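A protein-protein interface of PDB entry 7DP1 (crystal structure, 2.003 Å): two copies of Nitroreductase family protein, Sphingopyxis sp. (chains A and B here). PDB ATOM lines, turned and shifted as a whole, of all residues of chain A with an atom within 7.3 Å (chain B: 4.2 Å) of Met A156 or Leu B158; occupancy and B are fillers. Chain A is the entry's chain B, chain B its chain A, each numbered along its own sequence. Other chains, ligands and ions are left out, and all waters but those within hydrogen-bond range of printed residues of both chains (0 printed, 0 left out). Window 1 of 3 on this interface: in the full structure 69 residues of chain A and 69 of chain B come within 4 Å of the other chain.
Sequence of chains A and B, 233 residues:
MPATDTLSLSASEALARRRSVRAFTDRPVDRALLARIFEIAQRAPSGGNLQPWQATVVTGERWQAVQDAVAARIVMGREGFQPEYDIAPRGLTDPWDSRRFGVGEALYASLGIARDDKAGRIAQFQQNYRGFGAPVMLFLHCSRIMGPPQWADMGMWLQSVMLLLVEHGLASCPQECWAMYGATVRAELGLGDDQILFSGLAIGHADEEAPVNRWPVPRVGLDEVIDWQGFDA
Of the printed residues of chain B, Pro A45 touches Gln B159 (3.4 Å) and Met B162 (3.7 Å). Of the printed residues of chain B, Gly A155 touches Gly B155 (3.97 Å) and Met B156 (3.3 Å). Met A156 touches three residues of chain B. Of the printed residues of chain B, Gln A159 touches Met B156 (3.5 Å) and Ser B160 (2.9 Å). Printed residues of chain A within 4 Å of Gly B155: Ala A152, Gly A155 and Met A156. Of the printed residues of chain A, Gln B159 touches Pro A45, Met A156 and Ser A160. The nearest residue of chain A that does not touch Leu B158 is Pro A45 (6.6 Å). The nearest printed residue of chain B that does not touch Ala A152 is Met B156 (4.8 Å).
Gly B155 touches its own counterpart, Gly A155. Met A156 touches Leu B158, and with the chains exchanged Leu A158 touches Met B156. Met A156 touches Gln B159, and with the chains exchanged Gln A159 touches Met B156. Gln A159 touches Ser B160, and with the chains exchanged Ser A160 touches Gln B159.
Among the printed residues, merely in contact across the chains: Gly A155 with Met B156, Met A156 with Gly B155, Pro A45 with Gln B159, Ala A152 with Gly B155, Gln A159 with Met B156, Met A156 with Gln B159, Pro A45 with Met B162, Met A156 with Leu B158, Leu A158 with Met B156 and Gly A155 with Gly B155.
Hydrophobic or aromatic side chains of chain A that line the printed part of chain B: Pro A45, Met A156 and Leu A158. Hydrophobic or aromatic side chains of chain B within 4 Å of the printed part of chain A: Met B156, Leu B158 and Met B162. Among the printed residues, no Asp or Glu carboxylate lies within 4 Å of a Lys or Arg side-chain nitrogen of the other chain.
The side-chain hydroxyl of Ser B160 sits at hydrogen-bond distance from the side-chain amide nitrogen of Gln A159 (2.9 Å). The side-chain hydroxyl (OG) of Ser A160 is in hydrogen-bond range of the side-chain amide nitrogen (NE2) of Gln B159 (3.0 Å).
The backbone carbonyl oxygen of Met B156 lies within hydrogen-bond range of the side-chain hydroxyl of Ser B160. The side-chain hydroxyl of Ser A160 lies within hydrogen-bond range of the backbone carbonyl oxygen of Met A156.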
ATOM      1  N   ALA A  41      16.734  12.087  -6.593  1.00  0.00           N
ATOM      2  CA  ALA A  41      15.815  12.972  -5.882  1.00  0.00           C
ATOM      3  C   ALA A  41      15.967  14.436  -6.290  1.00  0.00           C
ATOM      4  O   ALA A  41      15.031  15.227  -6.168  1.00  0.00           O
ATOM      5  CB  ALA A  41      16.007  12.834  -4.373  1.00  0.00           C
ATOM      6  N   ALA A  44      13.479  16.263  -8.541  1.00  0.00           N
ATOM      7  CA  ALA A  44      12.230  16.863  -8.067  1.00  0.00           C
ATOM      8  C   ALA A  44      12.063  18.264  -8.665  1.00  0.00           C
ATOM      9  O   ALA A  44      13.034  18.995  -8.824  1.00  0.00           O
ATOM     10  CB  ALA A  44      12.218  16.932  -6.518  1.00  0.00           C
ATOM     11  N   PRO A  45      10.826  18.664  -8.967  1.00  0.00           N
ATOM     12  CA  PRO A  45      10.674  20.006  -9.528  1.00  0.00           C
ATOM     13  C   PRO A  45      10.737  21.078  -8.449  1.00  0.00           C
ATOM     14  O   PRO A  45      10.687  20.766  -7.268  1.00  0.00           O
ATOM     15  CB  PRO A  45       9.280  19.959 -10.146  1.00  0.00           C
ATOM     16  CG  PRO A  45       8.501  19.063  -9.168  1.00  0.00           C
ATOM     17  CD  PRO A  45       9.526  18.025  -8.681  1.00  0.00           C
ATOM     18  N   SER A  46      10.833  22.339  -8.852  1.00  0.00           N
ATOM     19  CA  SER A  46      10.748  23.425  -7.893  1.00  0.00           C
ATOM     20  C   SER A  46      10.381  24.647  -8.664  1.00  0.00           C
ATOM     21  O   SER A  46      10.747  24.772  -9.835  1.00  0.00           O
ATOM     22  CB  SER A  46      12.059  23.642  -7.135  1.00  0.00           C
ATOM     23  OG  SER A  46      13.121  23.984  -8.005  1.00  0.00           O
ATOM     24  N   GLY A  47       9.651  25.550  -8.016  1.00  0.00           N
ATOM     25  CA  GLY A  47       9.282  26.799  -8.665  1.00  0.00           C
ATOM     26  C   GLY A  47      10.532  27.453  -9.180  1.00  0.00           C
ATOM     27  O   GLY A  47      11.497  27.615  -8.441  1.00  0.00           O
ATOM     28  N   TRP A  53      16.026  23.207  -1.565  1.00  0.00           N
ATOM     29  CA  TRP A  53      16.373  22.302  -0.472  1.00  0.00           C
ATOM     30  C   TRP A  53      17.892  22.179  -0.261  1.00  0.00           C
ATOM     31  O   TRP A  53      18.673  22.172  -1.216  1.00  0.00           O
ATOM     32  CB  TRP A  53      15.783  20.903  -0.711  1.00  0.00           C
ATOM     33  CG  TRP A  53      16.070  20.356  -2.088  1.00  0.00           C
ATOM     34  CD1 TRP A  53      17.173  19.653  -2.481  1.00  0.00           C
ATOM     35  CD2 TRP A  53      15.232  20.467  -3.245  1.00  0.00           C
ATOM     36  NE1 TRP A  53      17.076  19.325  -3.813  1.00  0.00           N
ATOM     37  CE2 TRP A  53      15.880  19.796  -4.299  1.00  0.00           C
ATOM     38  CE3 TRP A  53      13.975  21.060  -3.488  1.00  0.00           C
ATOM     39  CZ2 TRP A  53      15.341  19.713  -5.586  1.00  0.00           C
ATOM     40  CZ3 TRP A  53      13.434  20.973  -4.767  1.00  0.00           C
ATOM     41  CH2 TRP A  53      14.118  20.305  -5.800  1.00  0.00           C
ATOM     42  N   PRO A 149       6.031  28.931  -0.836  1.00  0.00           N
ATOM     43  CA  PRO A 149       6.149  28.007  -1.976  1.00  0.00           C
ATOM     44  C   PRO A 149       7.500  27.247  -2.012  1.00  0.00           C
ATOM     45  O   PRO A 149       7.531  26.099  -2.457  1.00  0.00           O
ATOM     46  CB  PRO A 149       6.016  28.928  -3.185  1.00  0.00           C
ATOM     47  CG  PRO A 149       6.526  30.276  -2.681  1.00  0.00           C
ATOM     48  CD  PRO A 149       5.993  30.342  -1.271  1.00  0.00           C
ATOM     49  N   GLN A 150       8.588  27.859  -1.551  1.00  0.00           N
ATOM     50  CA  GLN A 150       9.869  27.137  -1.524  1.00  0.00           C
ATOM     51  C   GLN A 150       9.810  26.017  -0.486  1.00  0.00           C
ATOM     52  O   GLN A 150      10.326  24.925  -0.710  1.00  0.00           O
ATOM     53  CB  GLN A 150      11.030  28.079  -1.241  1.00  0.00           C
ATOM     54  CG  GLN A 150      11.440  28.863  -2.468  1.00  0.00           C
ATOM     55  CD  GLN A 150      10.478  30.001  -2.790  1.00  0.00           C
ATOM     56  OE1 GLN A 150      10.097  30.785  -1.914  1.00  0.00           O
ATOM     57  NE2 GLN A 150      10.062  30.076  -4.041  1.00  0.00           N
ATOM     58  N   TRP A 151       9.099  26.235   0.611  1.00  0.00           N
ATOM     59  CA  TRP A 151       8.907  25.138   1.557  1.00  0.00           C
ATOM     60  C   TRP A 151       8.120  24.032   0.876  1.00  0.00           C
ATOM     61  O   TRP A 151       8.334  22.851   1.152  1.00  0.00           O
ATOM     62  CB  TRP A 151       8.213  25.615   2.830  1.00  0.00           C
ATOM     63  CG  TRP A 151       9.191  26.254   3.767  1.00  0.00           C
ATOM     64  CD1 TRP A 151      10.057  27.284   3.483  1.00  0.00           C
ATOM     65  CD2 TRP A 151       9.410  25.914   5.138  1.00  0.00           C
ATOM     66  NE1 TRP A 151      10.806  27.592   4.599  1.00  0.00           N
ATOM     67  CE2 TRP A 151      10.429  26.764   5.626  1.00  0.00           C
ATOM     68  CE3 TRP A 151       8.848  24.974   6.004  1.00  0.00           C
ATOM     69  CZ2 TRP A 151      10.888  26.699   6.943  1.00  0.00           C
ATOM     70  CZ3 TRP A 151       9.315  24.909   7.315  1.00  0.00           C
ATOM     71  CH2 TRP A 151      10.322  25.769   7.771  1.00  0.00           C
ATOM     72  N   ALA A 152       7.203  24.388  -0.015  1.00  0.00           N
ATOM     73  CA  ALA A 152       6.491  23.332  -0.741  1.00  0.00           C
ATOM     74  C   ALA A 152       7.451  22.580  -1.658  1.00  0.00           C
ATOM     75  O   ALA A 152       7.360  21.353  -1.756  1.00  0.00           O
ATOM     76  CB  ALA A 152       5.285  23.894  -1.546  1.00  0.00           C
ATOM     77  N   ASP A 153       8.376  23.293  -2.300  1.00  0.00           N
ATOM     78  CA  ASP A 153       9.462  22.643  -3.092  1.00  0.00           C
ATOM     79  C   ASP A 153      10.272  21.638  -2.239  1.00  0.00           C
ATOM     80  O   ASP A 153      10.636  20.557  -2.703  1.00  0.00           O
ATOM     81  CB  ASP A 153      10.487  23.644  -3.642  1.00  0.00           C
ATOM     82  CG  ASP A 153       9.894  24.711  -4.583  1.00  0.00           C
ATOM     83  OD1 ASP A 153      10.549  25.776  -4.707  1.00  0.00           O
ATOM     84  OD2 ASP A 153       8.824  24.508  -5.195  1.00  0.00           O
ATOM     85  N   MET A 154      10.588  22.019  -1.002  1.00  0.00           N
ATOM     86  CA  MET A 154      11.310  21.121  -0.096  1.00  0.00           C
ATOM     87  C   MET A 154      10.486  19.870   0.154  1.00  0.00           C
ATOM     88  O   MET A 154      11.035  18.768   0.296  1.00  0.00           O
ATOM     89  CB  MET A 154      11.633  21.794   1.241  1.00  0.00           C
ATOM     90  CG  MET A 154      12.694  22.895   1.175  1.00  0.00           C
ATOM     91  SD  MET A 154      13.226  23.280   2.854  1.00  0.00           S
ATOM     92  CE  MET A 154      11.746  24.034   3.525  1.00  0.00           C
ATOM     93  N   GLY A 155       9.173  20.036   0.277  1.00  0.00           N
ATOM     94  CA  GLY A 155       8.309  18.866   0.424  1.00  0.00           C
ATOM     95  C   GLY A 155       8.402  17.902  -0.762  1.00  0.00           C
ATOM     96  O   GLY A 155       8.440  16.652  -0.611  1.00  0.00           O
ATOM     97  N   MET A 156       8.423  18.478  -1.957  1.00  0.00           N
ATOM     98  CA  MET A 156       8.535  17.684  -3.181  1.00  0.00           C
ATOM     99  C   MET A 156       9.813  16.838  -3.194  1.00  0.00           C
ATOM    100  O   MET A 156       9.789  15.644  -3.501  1.00  0.00           O
ATOM    101  CB  MET A 156       8.502  18.614  -4.400  1.00  0.00           C
ATOM    102  CG  MET A 156       7.136  19.267  -4.570  1.00  0.00           C
ATOM    103  SD  MET A 156       7.127  20.526  -5.864  1.00  0.00           S
ATOM    104  CE  MET A 156       5.729  21.513  -5.341  1.00  0.00           C
ATOM    105  N   TRP A 157      10.924  17.483  -2.857  1.00  0.00           N
ATOM    106  CA  TRP A 157      12.207  16.807  -2.760  1.00  0.00           C
ATOM    107  C   TRP A 157      12.136  15.724  -1.685  1.00  0.00           C
ATOM    108  O   TRP A 157      12.474  14.568  -1.935  1.00  0.00           O
ATOM    109  CB  TRP A 157      13.310  17.817  -2.436  1.00  0.00           C
ATOM    110  CG  TRP A 157      14.650  17.159  -2.310  1.00  0.00           C
ATOM    111  CD1 TRP A 157      15.476  16.787  -3.328  1.00  0.00           C
ATOM    112  CD2 TRP A 157      15.296  16.779  -1.100  1.00  0.00           C
ATOM    113  NE1 TRP A 157      16.613  16.203  -2.818  1.00  0.00           N
ATOM    114  CE2 TRP A 157      16.522  16.178  -1.453  1.00  0.00           C
ATOM    115  CE3 TRP A 157      14.961  16.887   0.247  1.00  0.00           C
ATOM    116  CZ2 TRP A 157      17.416  15.694  -0.510  1.00  0.00           C
ATOM    117  CZ3 TRP A 157      15.859  16.390   1.192  1.00  0.00           C
ATOM    118  CH2 TRP A 157      17.067  15.804   0.800  1.00  0.00           C
ATOM    119  N   LEU A 158      11.644  16.099  -0.508  1.00  0.00           N
ATOM    120  CA  LEU A 158      11.616  15.186   0.616  1.00  0.00           C
ATOM    121  C   LEU A 158      10.832  13.914   0.299  1.00  0.00           C
ATOM    122  O   LEU A 158      11.340  12.825   0.472  1.00  0.00           O
ATOM    123  CB  LEU A 158      11.041  15.874   1.863  1.00  0.00           C
ATOM    124  CG  LEU A 158      11.239  15.001   3.111  1.00  0.00           C
ATOM    125  CD1 LEU A 158      12.744  14.784   3.391  1.00  0.00           C
ATOM    126  CD2 LEU A 158      10.545  15.629   4.346  1.00  0.00           C
ATOM    127  N   GLN A 159       9.605  14.063  -0.206  1.00  0.00           N
ATOM    128  CA  GLN A 159       8.801  12.916  -0.598  1.00  0.00           C
ATOM    129  C   GLN A 159       9.495  12.121  -1.723  1.00  0.00           C
ATOM    130  O   GLN A 159       9.415  10.899  -1.771  1.00  0.00           O
ATOM    131  CB  GLN A 159       7.388  13.381  -1.021  1.00  0.00           C
ATOM    132  CG  GLN A 159       6.539  12.314  -1.703  1.00  0.00           C
ATOM    133  CD  GLN A 159       6.040  11.226  -0.738  1.00  0.00           C
ATOM    134  OE1 GLN A 159       6.638  10.980   0.328  1.00  0.00           O
ATOM    135  NE2 GLN A 159       4.930  10.573  -1.107  1.00  0.00           N
ATOM    136  N   SER A 160      10.203  12.802  -2.610  1.00  0.00           N
ATOM    137  CA  SER A 160      11.041  12.076  -3.594  1.00  0.00           C
ATOM    138  C   SER A 160      12.054  11.147  -2.887  1.00  0.00           C
ATOM    139  O   SER A 160      12.176   9.952  -3.207  1.00  0.00           O
ATOM    140  CB  SER A 160      11.794  13.049  -4.509  1.00  0.00           C
ATOM    141  OG  SER A 160      10.886  13.852  -5.256  1.00  0.00           O
ATOM    142  N   VAL A 161      12.737  11.684  -1.883  1.00  0.00           N
ATOM    143  CA  VAL A 161      13.719  10.895  -1.143  1.00  0.00           C
ATOM    144  C   VAL A 161      13.058   9.706  -0.454  1.00  0.00           C
ATOM    145  O   VAL A 161      13.528   8.569  -0.582  1.00  0.00           O
ATOM    146  CB  VAL A 161      14.433  11.758  -0.116  1.00  0.00           C
ATOM    147  CG1 VAL A 161      15.363  10.914   0.777  1.00  0.00           C
ATOM    148  CG2 VAL A 161      15.190  12.860  -0.839  1.00  0.00           C
ATOM    149  N   MET A 162      11.943   9.977   0.226  1.00  0.00           N
ATOM    150  CA  MET A 162      11.242   8.963   0.974  1.00  0.00           C
ATOM    151  C   MET A 162      10.778   7.812   0.095  1.00  0.00           C
ATOM    152  O   MET A 162      10.870   6.663   0.498  1.00  0.00           O
ATOM    153  CB  MET A 162      10.051   9.591   1.723  1.00  0.00           C
ATOM    154  CG  MET A 162      10.504  10.402   2.934  1.00  0.00           C
ATOM    155  SD  MET A 162       9.157  11.000   3.979  1.00  0.00           S
ATOM    156  CE  MET A 162       8.623  12.452   3.089  1.00  0.00           C
ATOM    157  N   LEU B 140      -4.504  23.608  -6.413  1.00  0.00           N
ATOM    158  CA  LEU B 140      -4.158  23.100  -5.090  1.00  0.00           C
ATOM    159  C   LEU B 140      -4.250  24.220  -4.095  1.00  0.00           C
ATOM    160  O   LEU B 140      -3.608  25.256  -4.260  1.00  0.00           O
ATOM    161  CB  LEU B 140      -2.744  22.475  -5.107  1.00  0.00           C
ATOM    162  CG  LEU B 140      -2.050  22.107  -3.787  1.00  0.00           C
ATOM    163  CD1 LEU B 140      -2.942  21.267  -2.901  1.00  0.00           C
ATOM    164  CD2 LEU B 140      -0.713  21.362  -4.077  1.00  0.00           C
ATOM    165  N   MET B 154       1.934  19.902   1.408  1.00  0.00           N
ATOM    166  CA  MET B 154       1.280  19.988   0.103  1.00  0.00           C
ATOM    167  C   MET B 154       2.224  19.570  -1.041  1.00  0.00           C
ATOM    168  O   MET B 154       1.800  18.891  -1.998  1.00  0.00           O
ATOM    169  CB  MET B 154       0.743  21.415  -0.151  1.00  0.00           C
ATOM    170  CG  MET B 154      -0.439  21.803   0.764  1.00  0.00           C
ATOM    171  SD  MET B 154      -1.333  23.285   0.196  1.00  0.00           S
ATOM    172  CE  MET B 154      -0.113  24.563   0.439  1.00  0.00           C
ATOM    173  N   GLY B 155       3.479  20.003  -0.952  1.00  0.00           N
ATOM    174  CA  GLY B 155       4.490  19.624  -1.941  1.00  0.00           C
ATOM    175  C   GLY B 155       4.638  18.116  -1.991  1.00  0.00           C
ATOM    176  O   GLY B 155       4.730  17.502  -3.056  1.00  0.00           O
ATOM    177  N   MET B 156       4.624  17.504  -0.820  1.00  0.00           N
ATOM    178  CA  MET B 156       4.754  16.050  -0.737  1.00  0.00           C
ATOM    179  C   MET B 156       3.627  15.416  -1.516  1.00  0.00           C
ATOM    180  O   MET B 156       3.846  14.497  -2.310  1.00  0.00           O
ATOM    181  CB  MET B 156       4.751  15.594   0.720  1.00  0.00           C
ATOM    182  CG  MET B 156       6.015  16.017   1.488  1.00  0.00           C
ATOM    183  SD  MET B 156       5.823  15.634   3.239  1.00  0.00           S
ATOM    184  CE  MET B 156       6.996  16.841   3.900  1.00  0.00           C
ATOM    185  N   TRP B 157       2.418  15.912  -1.296  1.00  0.00           N
ATOM    186  CA  TRP B 157       1.245  15.408  -2.046  1.00  0.00           C
ATOM    187  C   TRP B 157       1.352  15.677  -3.535  1.00  0.00           C
ATOM    188  O   TRP B 157       1.165  14.784  -4.362  1.00  0.00           O
ATOM    189  CB  TRP B 157      -0.036  16.028  -1.524  1.00  0.00           C
ATOM    190  CG  TRP B 157      -1.265  15.584  -2.262  1.00  0.00           C
ATOM    191  CD1 TRP B 157      -1.945  14.422  -2.068  1.00  0.00           C
ATOM    192  CD2 TRP B 157      -1.985  16.306  -3.288  1.00  0.00           C
ATOM    193  NE1 TRP B 157      -3.048  14.368  -2.896  1.00  0.00           N
ATOM    194  CE2 TRP B 157      -3.094  15.504  -3.660  1.00  0.00           C
ATOM    195  CE3 TRP B 157      -1.793  17.531  -3.933  1.00  0.00           C
ATOM    196  CZ2 TRP B 157      -4.029  15.894  -4.656  1.00  0.00           C
ATOM    197  CZ3 TRP B 157      -2.716  17.918  -4.928  1.00  0.00           C
ATOM    198  CH2 TRP B 157      -3.817  17.093  -5.276  1.00  0.00           C
ATOM    199  N   LEU B 158       1.656  16.921  -3.877  1.00  0.00           N
ATOM    200  CA  LEU B 158       1.746  17.314  -5.275  1.00  0.00           C
ATOM    201  C   LEU B 158       2.748  16.476  -6.047  1.00  0.00           C
ATOM    202  O   LEU B 158       2.469  16.035  -7.161  1.00  0.00           O
ATOM    203  CB  LEU B 158       2.128  18.803  -5.392  1.00  0.00           C
ATOM    204  CG  LEU B 158       1.963  19.306  -6.824  1.00  0.00           C
ATOM    205  CD1 LEU B 158       0.482  19.245  -7.239  1.00  0.00           C
ATOM    206  CD2 LEU B 158       2.516  20.708  -6.977  1.00  0.00           C
ATOM    207  N   GLN B 159       3.950  16.288  -5.485  1.00  0.00           N
ATOM    208  CA  GLN B 159       4.929  15.428  -6.150  1.00  0.00           C
ATOM    209  C   GLN B 159       4.419  13.985  -6.266  1.00  0.00           C
ATOM    210  O   GLN B 159       4.718  13.286  -7.226  1.00  0.00           O
ATOM    211  CB  GLN B 159       6.276  15.450  -5.405  1.00  0.00           C
ATOM    212  CG  GLN B 159       7.325  14.467  -5.935  1.00  0.00           C
ATOM    213  CD  GLN B 159       7.905  14.878  -7.284  1.00  0.00           C
ATOM    214  OE1 GLN B 159       7.274  15.616  -8.073  1.00  0.00           O
ATOM    215  NE2 GLN B 159       9.111  14.405  -7.565  1.00  0.00           N
ATOM    216  N   SER B 160       3.665  13.520  -5.279  1.00  0.00           N
ATOM    217  CA  SER B 160       3.044  12.197  -5.435  1.00  0.00           C
ATOM    218  C   SER B 160       2.167  12.161  -6.684  1.00  0.00           C
ATOM    219  O   SER B 160       2.256  11.225  -7.509  1.00  0.00           O
ATOM    220  CB  SER B 160       2.230  11.837  -4.197  1.00  0.00           C
ATOM    221  OG  SER B 160       3.086  11.773  -3.065  1.00  0.00           O
ATOM    222  N   VAL B 161       1.332  13.187  -6.852  1.00  0.00           N
ATOM    223  CA  VAL B 161       0.447  13.215  -8.023  1.00  0.00           C
ATOM    224  C   VAL B 161       1.230  13.239  -9.336  1.00  0.00           C
ATOM    225  O   VAL B 161       0.964  12.472 -10.261  1.00  0.00           O
ATOM    226  CB  VAL B 161      -0.498  14.425  -7.928  1.00  0.00           C
ATOM    227  CG1 VAL B 161      -1.343  14.574  -9.200  1.00  0.00           C
ATOM    228  CG2 VAL B 161      -1.375  14.264  -6.678  1.00  0.00           C
ATOM    229  N   MET B 162       2.228  14.108  -9.404  1.00  0.00           N
ATOM    230  CA  MET B 162       2.993  14.276 -10.628  1.00  0.00           C
ATOM    231  C   MET B 162       3.709  12.976 -11.030  1.00  0.00           C
ATOM    232  O   MET B 162       3.781  12.624 -12.203  1.00  0.00           O
ATOM    233  CB  MET B 162       3.994  15.413 -10.440  1.00  0.00           C
ATOM    234  CG  MET B 162       3.308  16.780 -10.350  1.00  0.00           C
ATOM    235  SD  MET B 162       4.536  18.086 -10.347  1.00  0.00           S
ATOM    236  CE  MET B 162       5.015  18.058  -8.631  1.00  0.00           C
ATOM    237  N   LEU B 201      -1.885  22.931 -11.307  1.00  0.00           N
ATOM    238  CA  LEU B 201      -1.150  21.831 -11.942  1.00  0.00           C
ATOM    239  C   LEU B 201      -1.848  21.522 -13.269  1.00  0.00           C
ATOM    240  O   LEU B 201      -2.965  20.999 -13.293  1.00  0.00           O
ATOM    241  CB  LEU B 201      -1.093  20.589 -11.037  1.00  0.00           C
ATOM    242  CG  LEU B 201      -0.368  19.328 -11.555  1.00  0.00           C
ATOM    243  CD1 LEU B 201       1.180  19.476 -11.528  1.00  0.00           C
ATOM    244  CD2 LEU B 201      -0.817  18.037 -10.817  1.00  0.00           C
